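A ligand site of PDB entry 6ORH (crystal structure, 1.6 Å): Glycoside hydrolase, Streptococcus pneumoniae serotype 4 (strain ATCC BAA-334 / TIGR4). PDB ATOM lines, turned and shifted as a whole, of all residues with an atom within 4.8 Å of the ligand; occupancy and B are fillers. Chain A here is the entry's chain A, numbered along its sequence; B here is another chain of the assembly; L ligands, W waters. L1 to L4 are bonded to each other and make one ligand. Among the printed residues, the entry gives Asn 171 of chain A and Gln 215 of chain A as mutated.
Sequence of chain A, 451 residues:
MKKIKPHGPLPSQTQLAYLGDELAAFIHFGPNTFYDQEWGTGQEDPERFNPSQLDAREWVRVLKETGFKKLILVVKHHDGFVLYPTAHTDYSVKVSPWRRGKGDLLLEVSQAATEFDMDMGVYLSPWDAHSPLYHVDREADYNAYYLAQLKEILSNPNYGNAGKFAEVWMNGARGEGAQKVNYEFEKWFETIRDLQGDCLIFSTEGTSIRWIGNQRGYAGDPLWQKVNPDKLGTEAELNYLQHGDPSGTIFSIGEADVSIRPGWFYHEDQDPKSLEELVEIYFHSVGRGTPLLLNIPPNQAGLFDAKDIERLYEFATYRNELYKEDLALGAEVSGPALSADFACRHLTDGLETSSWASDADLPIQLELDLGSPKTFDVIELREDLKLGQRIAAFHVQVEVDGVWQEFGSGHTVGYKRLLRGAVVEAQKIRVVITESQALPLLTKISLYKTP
An oxygen (O5) of LG2 L2 sits at hydrogen-bond distance from the side-chain carboxylate (OD2) of Asp 257 (2.6 Å). NE2 of Gln 215 lies within hydrogen-bond range of O5 of LG2 L2 (2.7 Å). A ring nitrogen (NE2) of His 28 sits at hydrogen-bond distance from an oxygen (O3) of LG4 L4 (2.8 Å). An oxygen (O1) of LG4 L4 sits at hydrogen-bond distance from a ring nitrogen (NE2) of His 78 (2.8 Å). NE1 of Trp 39 is in hydrogen-bond range of O1 of LG4 L4. An oxygen (O4) of LG4 L4 is in hydrogen-bond range of the side-chain amide nitrogen (ND2) of Asn 171, 2.8 Å away. An oxygen (O2) of LG4 L4 lies within hydrogen-bond range of a ring nitrogen (NE2) of His 77, 2.9 Å away. The side-chain hydroxyl of Tyr 123 lies within hydrogen-bond range of an oxygen (O3) of LG4 L4, 2.9 Å away. An oxygen (O3) of LG2 L2 is in hydrogen-bond range of the backbone NH (N) of Gly 172. An oxygen (O5) of LG2 L2 is in hydrogen-bond range of the indole nitrogen of Trp 211 (3.2 Å). The backbone carbonyl oxygen (O) of Thr 234 lies within hydrogen-bond range of an oxygen (O2) of LIG L1, at 3.3 Å.
The indole nitrogen (NE1) of Trp 211 is in hydrogen-bond range of the side-chain carboxylate (OD1) of Asp 257. The indole nitrogen (NE1) of Trp 264 is in hydrogen-bond range of the side-chain amide oxygen (OE1) of Gln 215, at 3.2 Å. N of Gln 215 lies within hydrogen-bond range of OE2 of Glu 406 of chain B (2.8 Å). The side-chain hydroxyl (OH) of Tyr 123 is in hydrogen-bond range of the side-chain amide nitrogen (ND2) of Asn 171, 3.0 Å away. OD1 of Asn 171 is in hydrogen-bond range of N of Ala 173 (2.9 Å). A ring nitrogen (NE2) of His 77 is in hydrogen-bond range of the side-chain hydroxyl of Tyr 123 (3.2 Å). The side-chain carboxylate (OE1) of Glu 235 lies within hydrogen-bond range of the side-chain hydroxyl (OG1) of Thr 234 (3.3 Å). The backbone NH (N) of Trp 264 lies within hydrogen-bond range of the side-chain carboxylate (OE1) of Glu 38 (2.9 Å).
Glu 38 touches the ligand. CH2 of Trp 169 touches C6 of LG2 L2, 3.5 Å away. CA of Ala 173 touches O4 of LIG L1, at 3.2 Å. N of Arg 174 touches C6 of LIG L1 (3.9 Å). Phe 202 touches the ligand. CG2 of Thr 204 touches O2 of LG2 L2, at 3.6 Å. NE1 of Trp 264 touches O5 of LG3 L3, 3.5 Å away. O of Trp 404 of chain B touches C1 of LG3 L3 (3.6 Å). Hydrophobic or aromatic side chains within 4 Å of the ligand: His 28, Trp 39, His 77, His 78, Tyr 123, Trp 169, Ala 173, Phe 202, Trp 211 and Trp 264. Of the 25 residues printed, 19 come within 4 Å of the ligand. Along chain A the residues within 4 Å of the ligand span positions 28 to 264. The nearest printed residue that does not touch the ligand is Phe 26 (4.02 Å).
Water W7 lies within hydrogen-bond range of the backbone carbonyl oxygen of Trp 404 of chain B and an oxygen (O6) of LG3 L3. Water W1 bridges O2 of LG4 L4 (2.7 Å) and O of Glu 38 (2.8 Å). Water W6 lies within hydrogen-bond range of the backbone carbonyl oxygen of Gly 172, an oxygen (O3) of LIG L1 and the backbone NH of Arg 174. Water W9 lies within hydrogen-bond range of the backbone carbonyl oxygen of Trp 404 of chain B, an oxygen (O4) of LG3 L3 and the backbone NH of Glu 406 of chain B. Water W8 bridges the backbone carbonyl oxygen of Thr 234 and an oxygen (O1) of LIG L1.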
ATOM      1  N   PHE A  26      -1.312 -20.358  18.379  1.00  0.00           N
ATOM      2  CA  PHE A  26      -0.896 -19.216  19.180  1.00  0.00           C
ATOM      3  C   PHE A  26      -1.277 -19.521  20.629  1.00  0.00           C
ATOM      4  O   PHE A  26      -2.310 -20.160  20.861  1.00  0.00           O
ATOM      5  CB  PHE A  26      -1.743 -18.019  18.771  1.00  0.00           C
ATOM      6  CG  PHE A  26      -1.060 -16.695  18.473  1.00  0.00           C
ATOM      7  CD1 PHE A  26       0.194 -16.351  18.971  1.00  0.00           C
ATOM      8  CD2 PHE A  26      -1.766 -15.738  17.745  1.00  0.00           C
ATOM      9  CE1 PHE A  26       0.754 -15.121  18.695  1.00  0.00           C
ATOM     10  CE2 PHE A  26      -1.205 -14.507  17.456  1.00  0.00           C
ATOM     11  CZ  PHE A  26       0.056 -14.192  17.939  1.00  0.00           C
ATOM     12  N   HIS A  28      -1.836 -17.266  24.046  1.00  0.00           N
ATOM     13  CA  HIS A  28      -1.892 -16.059  24.873  1.00  0.00           C
ATOM     14  C   HIS A  28      -2.234 -16.492  26.298  1.00  0.00           C
ATOM     15  O   HIS A  28      -3.316 -17.014  26.538  1.00  0.00           O
ATOM     16  CB  HIS A  28      -2.961 -15.045  24.384  1.00  0.00           C
ATOM     17  CG  HIS A  28      -2.579 -14.240  23.178  1.00  0.00           C
ATOM     18  ND1 HIS A  28      -2.454 -14.812  21.918  1.00  0.00           N
ATOM     19  CD2 HIS A  28      -2.352 -12.913  23.025  1.00  0.00           C
ATOM     20  CE1 HIS A  28      -2.148 -13.846  21.041  1.00  0.00           C
ATOM     21  NE2 HIS A  28      -2.092 -12.682  21.700  1.00  0.00           N
ATOM     22  N   GLU A  38      -8.356  -8.384  28.349  1.00  0.00           N
ATOM     23  CA  GLU A  38      -7.708  -8.611  27.051  1.00  0.00           C
ATOM     24  C   GLU A  38      -6.405  -7.825  26.967  1.00  0.00           C
ATOM     25  O   GLU A  38      -5.429  -8.293  26.372  1.00  0.00           O
ATOM     26  CB  GLU A  38      -8.658  -8.288  25.908  1.00  0.00           C
ATOM     27  CG  GLU A  38      -9.662  -9.401  25.673  1.00  0.00           C
ATOM     28  CD  GLU A  38      -8.975 -10.615  25.064  1.00  0.00           C
ATOM     29  OE1 GLU A  38      -8.555 -10.521  23.900  1.00  0.00           O
ATOM     30  OE2 GLU A  38      -8.866 -11.664  25.737  1.00  0.00           O
ATOM     31  N   TRP A  39      -6.386  -6.621  27.567  1.00  0.00           N
ATOM     32  CA  TRP A  39      -5.163  -5.833  27.645  1.00  0.00           C
ATOM     33  C   TRP A  39      -4.895  -5.496  29.109  1.00  0.00           C
ATOM     34  O   TRP A  39      -5.847  -5.239  29.845  1.00  0.00           O
ATOM     35  CB  TRP A  39      -5.319  -4.506  26.869  1.00  0.00           C
ATOM     36  CG  TRP A  39      -5.121  -4.569  25.391  1.00  0.00           C
ATOM     37  CD1 TRP A  39      -4.948  -5.685  24.598  1.00  0.00           C
ATOM     38  CD2 TRP A  39      -5.096  -3.432  24.490  1.00  0.00           C
ATOM     39  NE1 TRP A  39      -4.824  -5.313  23.279  1.00  0.00           N
ATOM     40  CE2 TRP A  39      -4.902  -3.941  23.186  1.00  0.00           C
ATOM     41  CE3 TRP A  39      -5.210  -2.040  24.672  1.00  0.00           C
ATOM     42  CZ2 TRP A  39      -4.831  -3.100  22.073  1.00  0.00           C
ATOM     43  CZ3 TRP A  39      -5.114  -1.225  23.568  1.00  0.00           C
ATOM     44  CH2 TRP A  39      -4.926  -1.749  22.290  1.00  0.00           C
ATOM     45  N   HIS A  77       3.253  -9.785  26.866  1.00  0.00           N
ATOM     46  CA  HIS A  77       2.189  -9.072  26.159  1.00  0.00           C
ATOM     47  C   HIS A  77       2.345  -7.577  26.408  1.00  0.00           C
ATOM     48  O   HIS A  77       3.366  -7.155  26.932  1.00  0.00           O
ATOM     49  CB  HIS A  77       0.819  -9.655  26.575  1.00  0.00           C
ATOM     50  CG  HIS A  77      -0.239  -9.395  25.558  1.00  0.00           C
ATOM     51  ND1 HIS A  77      -1.175  -8.387  25.726  1.00  0.00           N
ATOM     52  CD2 HIS A  77      -0.525  -9.982  24.377  1.00  0.00           C
ATOM     53  CE1 HIS A  77      -1.982  -8.368  24.689  1.00  0.00           C
ATOM     54  NE2 HIS A  77      -1.619  -9.328  23.842  1.00  0.00           N
ATOM     55  N   HIS A  78       1.347  -6.772  26.014  1.00  0.00           N
ATOM     56  CA  HIS A  78       1.499  -5.322  26.117  1.00  0.00           C
ATOM     57  C   HIS A  78       1.690  -4.862  27.572  1.00  0.00           C
ATOM     58  O   HIS A  78       2.308  -3.829  27.820  1.00  0.00           O
ATOM     59  CB  HIS A  78       0.230  -4.620  25.578  1.00  0.00           C
ATOM     60  CG  HIS A  78      -0.214  -5.025  24.210  1.00  0.00           C
ATOM     61  ND1 HIS A  78       0.666  -5.294  23.158  1.00  0.00           N
ATOM     62  CD2 HIS A  78      -1.465  -5.145  23.704  1.00  0.00           C
ATOM     63  CE1 HIS A  78      -0.054  -5.590  22.071  1.00  0.00           C
ATOM     64  NE2 HIS A  78      -1.361  -5.504  22.369  1.00  0.00           N
ATOM     65  N   TYR A 123       6.491 -14.429  20.755  1.00  0.00           N
ATOM     66  CA  TYR A 123       5.805 -13.129  20.656  1.00  0.00           C
ATOM     67  C   TYR A 123       6.300 -12.276  21.806  1.00  0.00           C
ATOM     68  O   TYR A 123       6.122 -12.647  22.969  1.00  0.00           O
ATOM     69  CB  TYR A 123       4.293 -13.357  20.669  1.00  0.00           C
ATOM     70  CG  TYR A 123       3.339 -12.180  20.837  1.00  0.00           C
ATOM     71  CD1 TYR A 123       3.434 -11.311  21.919  1.00  0.00           C
ATOM     72  CD2 TYR A 123       2.223 -12.105  20.009  1.00  0.00           C
ATOM     73  CE1 TYR A 123       2.528 -10.270  22.057  1.00  0.00           C
ATOM     74  CE2 TYR A 123       1.277 -11.101  20.169  1.00  0.00           C
ATOM     75  CZ  TYR A 123       1.429 -10.181  21.203  1.00  0.00           C
ATOM     76  OH  TYR A 123       0.490  -9.206  21.426  1.00  0.00           O
ATOM     77  N   TRP A 169       7.344 -12.764  16.560  1.00  0.00           N
ATOM     78  CA  TRP A 169       6.141 -11.958  16.363  1.00  0.00           C
ATOM     79  C   TRP A 169       6.330 -10.595  17.014  1.00  0.00           C
ATOM     80  O   TRP A 169       6.555 -10.499  18.238  1.00  0.00           O
ATOM     81  CB  TRP A 169       4.943 -12.693  17.004  1.00  0.00           C
ATOM     82  CG  TRP A 169       3.828 -12.997  16.040  1.00  0.00           C
ATOM     83  CD1 TRP A 169       3.805 -13.992  15.102  1.00  0.00           C
ATOM     84  CD2 TRP A 169       2.554 -12.331  15.956  1.00  0.00           C
ATOM     85  NE1 TRP A 169       2.619 -13.987  14.419  1.00  0.00           N
ATOM     86  CE2 TRP A 169       1.821 -13.013  14.951  1.00  0.00           C
ATOM     87  CE3 TRP A 169       1.957 -11.248  16.632  1.00  0.00           C
ATOM     88  CZ2 TRP A 169       0.529 -12.639  14.590  1.00  0.00           C
ATOM     89  CZ3 TRP A 169       0.653 -10.924  16.302  1.00  0.00           C
ATOM     90  CH2 TRP A 169      -0.030 -11.577  15.256  1.00  0.00           C
ATOM     91  N   ASN A 171       4.012  -7.596  17.389  1.00  0.00           N
ATOM     92  CA  ASN A 171       2.664  -7.065  17.266  1.00  0.00           C
ATOM     93  C   ASN A 171       2.723  -5.567  16.990  1.00  0.00           C
ATOM     94  O   ASN A 171       3.521  -4.873  17.611  1.00  0.00           O
ATOM     95  CB  ASN A 171       1.914  -7.340  18.580  1.00  0.00           C
ATOM     96  CG  ASN A 171       0.426  -7.309  18.369  1.00  0.00           C
ATOM     97  OD1 ASN A 171      -0.144  -6.267  18.062  1.00  0.00           O
ATOM     98  ND2 ASN A 171      -0.217  -8.431  18.569  1.00  0.00           N
ATOM     99  N   GLY A 172       1.855  -5.062  16.081  1.00  0.00           N
ATOM    100  CA  GLY A 172       1.874  -3.627  15.781  1.00  0.00           C
ATOM    101  C   GLY A 172       0.949  -2.788  16.676  1.00  0.00           C
ATOM    102  O   GLY A 172       0.958  -1.567  16.548  1.00  0.00           O
ATOM    103  N   ALA A 173       0.211  -3.424  17.599  1.00  0.00           N
ATOM    104  CA  ALA A 173      -0.824  -2.735  18.379  1.00  0.00           C
ATOM    105  C   ALA A 173      -0.213  -1.848  19.466  1.00  0.00           C
ATOM    106  O   ALA A 173       0.695  -2.258  20.186  1.00  0.00           O
ATOM    107  CB  ALA A 173      -1.786  -3.737  18.997  1.00  0.00           C
ATOM    108  N   ARG A 174      -0.765  -0.622  19.607  1.00  0.00           N
ATOM    109  CA  ARG A 174      -0.405   0.246  20.713  1.00  0.00           C
ATOM    110  C   ARG A 174      -1.625   1.080  21.101  1.00  0.00           C
ATOM    111  O   ARG A 174      -2.368   1.508  20.224  1.00  0.00           O
ATOM    112  CB  ARG A 174       0.742   1.159  20.304  1.00  0.00           C
ATOM    113  CG  ARG A 174       1.194   2.119  21.392  1.00  0.00           C
ATOM    114  CD  ARG A 174       2.561   2.707  21.197  1.00  0.00           C
ATOM    115  NE  ARG A 174       2.573   3.573  20.014  1.00  0.00           N
ATOM    116  CZ  ARG A 174       3.645   3.890  19.305  1.00  0.00           C
ATOM    117  NH1 ARG A 174       4.841   3.447  19.664  1.00  0.00           N
ATOM    118  NH2 ARG A 174       3.516   4.685  18.244  1.00  0.00           N
ATOM    119  N   PHE A 202       7.049 -11.776  11.802  1.00  0.00           N
ATOM    120  CA  PHE A 202       5.796 -11.036  11.653  1.00  0.00           C
ATOM    121  C   PHE A 202       6.008  -9.644  12.237  1.00  0.00           C
ATOM    122  O   PHE A 202       6.443  -9.515  13.381  1.00  0.00           O
ATOM    123  CB  PHE A 202       4.705 -11.755  12.472  1.00  0.00           C
ATOM    124  CG  PHE A 202       3.367 -11.068  12.452  1.00  0.00           C
ATOM    125  CD1 PHE A 202       3.137  -9.939  13.225  1.00  0.00           C
ATOM    126  CD2 PHE A 202       2.331 -11.552  11.666  1.00  0.00           C
ATOM    127  CE1 PHE A 202       1.896  -9.322  13.220  1.00  0.00           C
ATOM    128  CE2 PHE A 202       1.082 -10.932  11.645  1.00  0.00           C
ATOM    129  CZ  PHE A 202       0.874  -9.800  12.414  1.00  0.00           C
ATOM    130  N   THR A 204       4.955  -5.053  11.309  1.00  0.00           N
ATOM    131  CA  THR A 204       4.322  -4.044  10.479  1.00  0.00           C
ATOM    132  C   THR A 204       5.186  -3.635   9.293  1.00  0.00           C
ATOM    133  O   THR A 204       4.690  -2.943   8.411  1.00  0.00           O
ATOM    134  CB  THR A 204       3.961  -2.816  11.320  1.00  0.00           C
ATOM    135  OG1 THR A 204       5.115  -2.303  12.008  1.00  0.00           O
ATOM    136  CG2 THR A 204       2.827  -3.099  12.281  1.00  0.00           C
ATOM    137  N   TRP A 211       0.570  -9.130   8.579  1.00  0.00           N
ATOM    138  CA  TRP A 211      -0.778  -9.374   9.031  1.00  0.00           C
ATOM    139  C   TRP A 211      -1.739  -9.443   7.843  1.00  0.00           C
ATOM    140  O   TRP A 211      -1.549  -8.687   6.889  1.00  0.00           O
ATOM    141  CB  TRP A 211      -1.126  -8.230   9.984  1.00  0.00           C
ATOM    142  CG  TRP A 211      -2.430  -8.493  10.662  1.00  0.00           C
ATOM    143  CD1 TRP A 211      -2.930  -9.691  11.103  1.00  0.00           C
ATOM    144  CD2 TRP A 211      -3.405  -7.497  10.974  1.00  0.00           C
ATOM    145  NE1 TRP A 211      -4.163  -9.503  11.666  1.00  0.00           N
ATOM    146  CE2 TRP A 211      -4.479  -8.176  11.612  1.00  0.00           C
ATOM    147  CE3 TRP A 211      -3.472  -6.114  10.804  1.00  0.00           C
ATOM    148  CZ2 TRP A 211      -5.606  -7.503  12.080  1.00  0.00           C
ATOM    149  CZ3 TRP A 211      -4.589  -5.442  11.273  1.00  0.00           C
ATOM    150  CH2 TRP A 211      -5.643  -6.137  11.884  1.00  0.00           C
ATOM    151  N   GLN A 215      -8.703 -10.255  12.278  1.00  0.00           N
ATOM    152  CA  GLN A 215      -8.496 -11.337  13.224  1.00  0.00           C
ATOM    153  C   GLN A 215      -9.645 -12.332  13.122  1.00  0.00           C
ATOM    154  O   GLN A 215     -10.005 -12.980  14.125  1.00  0.00           O
ATOM    155  CB  GLN A 215      -8.310 -10.765  14.635  1.00  0.00           C
ATOM    156  CG  GLN A 215      -7.150  -9.777  14.717  1.00  0.00           C
ATOM    157  CD  GLN A 215      -6.939  -9.162  16.076  1.00  0.00           C
ATOM    158  OE1 GLN A 215      -7.833  -9.177  16.924  1.00  0.00           O
ATOM    159  NE2 GLN A 215      -5.731  -8.673  16.320  1.00  0.00           N
ATOM    160  N   THR A 234       2.295   0.801  10.197  1.00  0.00           N
ATOM    161  CA  THR A 234       1.072   0.701  10.994  1.00  0.00           C
ATOM    162  C   THR A 234      -0.184   1.206  10.267  1.00  0.00           C
ATOM    163  O   THR A 234      -1.289   0.781  10.610  1.00  0.00           O
ATOM    164  CB  THR A 234       1.236   1.352  12.378  1.00  0.00           C
ATOM    165  OG1 THR A 234       1.661   2.698  12.144  1.00  0.00           O
ATOM    166  CG2 THR A 234       2.310   0.700  13.203  1.00  0.00           C
ATOM    167  N   GLU A 235      -0.005   2.090   9.270  1.00  0.00           N
ATOM    168  CA  GLU A 235      -1.129   2.624   8.510  1.00  0.00           C
ATOM    169  C   GLU A 235      -1.258   1.956   7.151  1.00  0.00           C
ATOM    170  O   GLU A 235      -1.796   2.566   6.223  1.00  0.00           O
ATOM    171  CB  GLU A 235      -0.949   4.132   8.270  1.00  0.00           C
ATOM    172  CG  GLU A 235      -0.698   4.906   9.544  1.00  0.00           C
ATOM    173  CD  GLU A 235      -1.707   4.527  10.607  1.00  0.00           C
ATOM    174  OE1 GLU A 235      -1.287   4.136  11.697  1.00  0.00           O
ATOM    175  OE2 GLU A 235      -2.922   4.587  10.287  1.00  0.00           O
ATOM    176  N   ASP A 257      -4.347 -14.884  11.594  1.00  0.00           N
ATOM    177  CA  ASP A 257      -4.428 -15.199  13.007  1.00  0.00           C
ATOM    178  C   ASP A 257      -5.848 -15.007  13.498  1.00  0.00           C
ATOM    179  O   ASP A 257      -6.521 -14.043  13.146  1.00  0.00           O
ATOM    180  CB  ASP A 257      -3.451 -14.323  13.817  1.00  0.00           C
ATOM    181  CG  ASP A 257      -3.705 -12.815  13.710  1.00  0.00           C
ATOM    182  OD1 ASP A 257      -4.008 -12.320  12.576  1.00  0.00           O
ATOM    183  OD2 ASP A 257      -3.607 -12.122  14.732  1.00  0.00           O
ATOM    184  N   TRP A 264      -8.498 -13.222  22.987  1.00  0.00           N
ATOM    185  CA  TRP A 264      -7.199 -13.883  22.854  1.00  0.00           C
ATOM    186  C   TRP A 264      -6.824 -14.593  24.155  1.00  0.00           C
ATOM    187  O   TRP A 264      -6.177 -15.643  24.122  1.00  0.00           O
ATOM    188  CB  TRP A 264      -6.124 -12.850  22.478  1.00  0.00           C
ATOM    189  CG  TRP A 264      -6.357 -12.221  21.132  1.00  0.00           C
ATOM    190  CD1 TRP A 264      -6.937 -11.006  20.848  1.00  0.00           C
ATOM    191  CD2 TRP A 264      -6.055 -12.833  19.870  1.00  0.00           C
ATOM    192  NE1 TRP A 264      -6.990 -10.821  19.490  1.00  0.00           N
ATOM    193  CE2 TRP A 264      -6.498 -11.946  18.856  1.00  0.00           C
ATOM    194  CE3 TRP A 264      -5.476 -14.053  19.497  1.00  0.00           C
ATOM    195  CZ2 TRP A 264      -6.306 -12.234  17.506  1.00  0.00           C
ATOM    196  CZ3 TRP A 264      -5.321 -14.357  18.164  1.00  0.00           C
ATOM    197  CH2 TRP A 264      -5.711 -13.439  17.187  1.00  0.00           C
ATOM    198  N   GLN B 397     -15.482  -0.666  13.531  1.00  0.00           N
ATOM    199  CA  GLN B 397     -14.971  -1.105  14.829  1.00  0.00           C
ATOM    200  C   GLN B 397     -16.052  -0.914  15.881  1.00  0.00           C
ATOM    201  O   GLN B 397     -16.945  -0.088  15.701  1.00  0.00           O
ATOM    202  CB  GLN B 397     -13.814  -0.197  15.270  1.00  0.00           C
ATOM    203  CG  GLN B 397     -12.708  -0.130  14.258  1.00  0.00           C
ATOM    204  CD  GLN B 397     -11.557   0.719  14.737  1.00  0.00           C
ATOM    205  OE1 GLN B 397     -10.406   0.430  14.465  1.00  0.00           O
ATOM    206  NE2 GLN B 397     -11.882   1.766  15.494  1.00  0.00           N
ATOM    207  N   VAL B 403     -11.624  -1.355  24.666  1.00  0.00           N
ATOM    208  CA  VAL B 403     -10.726  -1.584  23.526  1.00  0.00           C
ATOM    209  C   VAL B 403     -11.525  -1.566  22.226  1.00  0.00           C
ATOM    210  O   VAL B 403     -12.515  -2.286  22.101  1.00  0.00           O
ATOM    211  CB  VAL B 403      -9.967  -2.920  23.639  1.00  0.00           C
ATOM    212  CG1 VAL B 403      -8.913  -3.066  22.536  1.00  0.00           C
ATOM    213  CG2 VAL B 403      -9.347  -3.127  25.020  1.00  0.00           C
ATOM    214  N   TRP B 404     -11.058  -0.775  21.251  1.00  0.00           N
ATOM    215  CA  TRP B 404     -11.697  -0.729  19.943  1.00  0.00           C
ATOM    216  C   TRP B 404     -11.302  -1.966  19.148  1.00  0.00           C
ATOM    217  O   TRP B 404     -10.119  -2.165  18.835  1.00  0.00           O
ATOM    218  CB  TRP B 404     -11.340   0.564  19.190  1.00  0.00           C
ATOM    219  CG  TRP B 404     -12.067   1.747  19.736  1.00  0.00           C
ATOM    220  CD1 TRP B 404     -11.608   2.655  20.657  1.00  0.00           C
ATOM    221  CD2 TRP B 404     -13.422   2.137  19.419  1.00  0.00           C
ATOM    222  NE1 TRP B 404     -12.583   3.575  20.929  1.00  0.00           N
ATOM    223  CE2 TRP B 404     -13.707   3.291  20.186  1.00  0.00           C
ATOM    224  CE3 TRP B 404     -14.417   1.627  18.585  1.00  0.00           C
ATOM    225  CZ2 TRP B 404     -14.932   3.954  20.114  1.00  0.00           C
ATOM    226  CZ3 TRP B 404     -15.632   2.281  18.507  1.00  0.00           C
ATOM    227  CH2 TRP B 404     -15.886   3.430  19.264  1.00  0.00           C
ATOM    228  N   GLN B 405     -12.305  -2.799  18.844  1.00  0.00           N
ATOM    229  CA  GLN B 405     -12.052  -4.089  18.221  1.00  0.00           C
ATOM    230  C   GLN B 405     -12.712  -4.077  16.852  1.00  0.00           C
ATOM    231  O   GLN B 405     -13.661  -3.359  16.609  1.00  0.00           O
ATOM    232  CB  GLN B 405     -12.605  -5.211  19.103  1.00  0.00           C
ATOM    233  CG  GLN B 405     -11.713  -5.477  20.321  1.00  0.00           C
ATOM    234  CD  GLN B 405     -12.237  -6.498  21.312  1.00  0.00           C
ATOM    235  OE1 GLN B 405     -11.642  -6.696  22.370  1.00  0.00           O
ATOM    236  NE2 GLN B 405     -13.351  -7.134  20.978  1.00  0.00           N
ATOM    237  N   GLU B 406     -12.182  -4.867  15.914  1.00  0.00           N
ATOM    238  CA  GLU B 406     -12.778  -4.814  14.597  1.00  0.00           C
ATOM    239  C   GLU B 406     -14.100  -5.571  14.631  1.00  0.00           C
ATOM    240  O   GLU B 406     -14.298  -6.519  15.394  1.00  0.00           O
ATOM    241  CB  GLU B 406     -11.803  -5.376  13.554  1.00  0.00           C
ATOM    242  CG  GLU B 406     -11.064  -6.546  14.159  1.00  0.00           C
ATOM    243  CD  GLU B 406     -10.265  -7.423  13.226  1.00  0.00           C
ATOM    244  OE1 GLU B 406      -9.077  -7.062  12.947  1.00  0.00           O
ATOM    245  OE2 GLU B 406     -10.804  -8.476  12.872  1.00  0.00           O
HETATM  246  C1  LIG L   1      -1.991  -2.298  14.705  1.00  0.00           C
HETATM  247  C2  LIG L   1      -2.148  -1.281  13.561  1.00  0.00           C
HETATM  248  C3  LIG L   1      -3.601  -0.740  13.569  1.00  0.00           C
HETATM  249  C4  LIG L   1      -3.940  -0.120  14.906  1.00  0.00           C
HETATM  250  C5  LIG L   1      -3.766  -1.198  15.970  1.00  0.00           C
HETATM  251  C6  LIG L   1      -4.029  -0.715  17.393  1.00  0.00           C
HETATM  252  O1  LIG L   1      -1.848  -1.925  12.354  1.00  0.00           O
HETATM  253  O2  LIG L   1      -3.842   0.233  12.548  1.00  0.00           O
HETATM  254  O3  LIG L   1      -3.087   0.994  15.215  1.00  0.00           O
HETATM  255  O4  LIG L   1      -2.419  -1.641  15.884  1.00  0.00           O
HETATM  256  C1  LG2 L   2      -3.438  -5.578  15.269  1.00  0.00           C
HETATM  257  C2  LG2 L   2      -2.245  -4.688  14.864  1.00  0.00           C
HETATM  258  C3  LG2 L   2      -1.391  -5.362  13.793  1.00  0.00           C
HETATM  259  C4  LG2 L   2      -1.122  -6.839  14.110  1.00  0.00           C
HETATM  260  C5  LG2 L   2      -2.467  -7.512  14.416  1.00  0.00           C
HETATM  261  C6  LG2 L   2      -2.354  -8.989  14.743  1.00  0.00           C
HETATM  262  O1  LG2 L   2      -2.751  -3.451  14.319  1.00  0.00           O
HETATM  263  O2  LG2 L   2      -0.149  -4.628  13.598  1.00  0.00           O
HETATM  264  O3  LG2 L   2      -0.240  -6.983  15.262  1.00  0.00           O
HETATM  265  O4  LG2 L   2      -2.996  -6.888  15.616  1.00  0.00           O
HETATM  266  O5  LG2 L   2      -3.690  -9.556  14.786  1.00  0.00           O
HETATM  267  C1  LG3 L   3      -7.344  -4.413  18.644  1.00  0.00           C
HETATM  268  C2  LG3 L   3      -6.696  -5.781  18.870  1.00  0.00           C
HETATM  269  C3  LG3 L   3      -5.276  -5.801  18.310  1.00  0.00           C
HETATM  270  C4  LG3 L   3      -5.261  -5.351  16.812  1.00  0.00           C
HETATM  271  C5  LG3 L   3      -6.076  -4.053  16.669  1.00  0.00           C
HETATM  272  C6  LG3 L   3      -6.361  -3.941  15.150  1.00  0.00           C
HETATM  273  C7  LG3 L   3      -7.569  -6.995  20.842  1.00  0.00           C
HETATM  274  C8  LG3 L   3      -7.573  -7.130  22.346  1.00  0.00           C
HETATM  275  O1  LG3 L   3      -7.399  -4.178  17.203  1.00  0.00           O
HETATM  276  O2  LG3 L   3      -4.769  -7.157  18.442  1.00  0.00           O
HETATM  277  O3  LG3 L   3      -3.901  -5.007  16.524  1.00  0.00           O
HETATM  278  O4  LG3 L   3      -6.933  -2.671  14.885  1.00  0.00           O
HETATM  279  O5  LG3 L   3      -8.327  -7.639  20.136  1.00  0.00           O
HETATM  280  N1  LG3 L   3      -6.727  -6.086  20.310  1.00  0.00           N
HETATM  281  O6  LG3 L   3      -6.583  -3.399  19.243  1.00  0.00           O
HETATM  282  C1  LG4 L   4      -3.444  -7.338  18.846  1.00  0.00           C
HETATM  283  C2  LG4 L   4      -3.188  -7.356  20.338  1.00  0.00           C
HETATM  284  C3  LG4 L   4      -4.018  -8.475  20.944  1.00  0.00           C
HETATM  285  C4  LG4 L   4      -3.550  -9.826  20.401  1.00  0.00           C
HETATM  286  C5  LG4 L   4      -3.663  -9.788  18.856  1.00  0.00           C
HETATM  287  C6  LG4 L   4      -3.046 -11.015  18.209  1.00  0.00           C
HETATM  288  O1  LG4 L   4      -3.607  -6.077  20.862  1.00  0.00           O
HETATM  289  O2  LG4 L   4      -3.899  -8.440  22.373  1.00  0.00           O
HETATM  290  O3  LG4 L   4      -2.180 -10.063  20.851  1.00  0.00           O
HETATM  291  O4  LG4 L   4      -3.015  -8.587  18.283  1.00  0.00           O
HETATM  292  O   HOH W   1      -5.746  -9.719  23.947  1.00  0.00           O
HETATM  293  O   HOH W   2     -10.076  -9.351  21.996  1.00  0.00           O
HETATM  294  O   HOH W   3      -0.160  -2.797   9.459  1.00  0.00           O
HETATM  295  O   HOH W   4      -8.002  -2.726  12.250  1.00  0.00           O
HETATM  296  O   HOH W   5       0.204  -5.129  10.929  1.00  0.00           O
HETATM  297  O   HOH W   6      -0.665   0.759  16.746  1.00  0.00           O
HETATM  298  O   HOH W   7      -7.796  -1.052  19.384  1.00  0.00           O
HETATM  299  O   HOH W   8      -2.651  -1.496   9.180  1.00  0.00           O
HETATM  300  O   HOH W   9      -9.767  -2.741  15.941  1.00  0.00           O
HETATM  301  O   HOH W  10      -6.605  -0.505  11.163  1.00  0.00           O
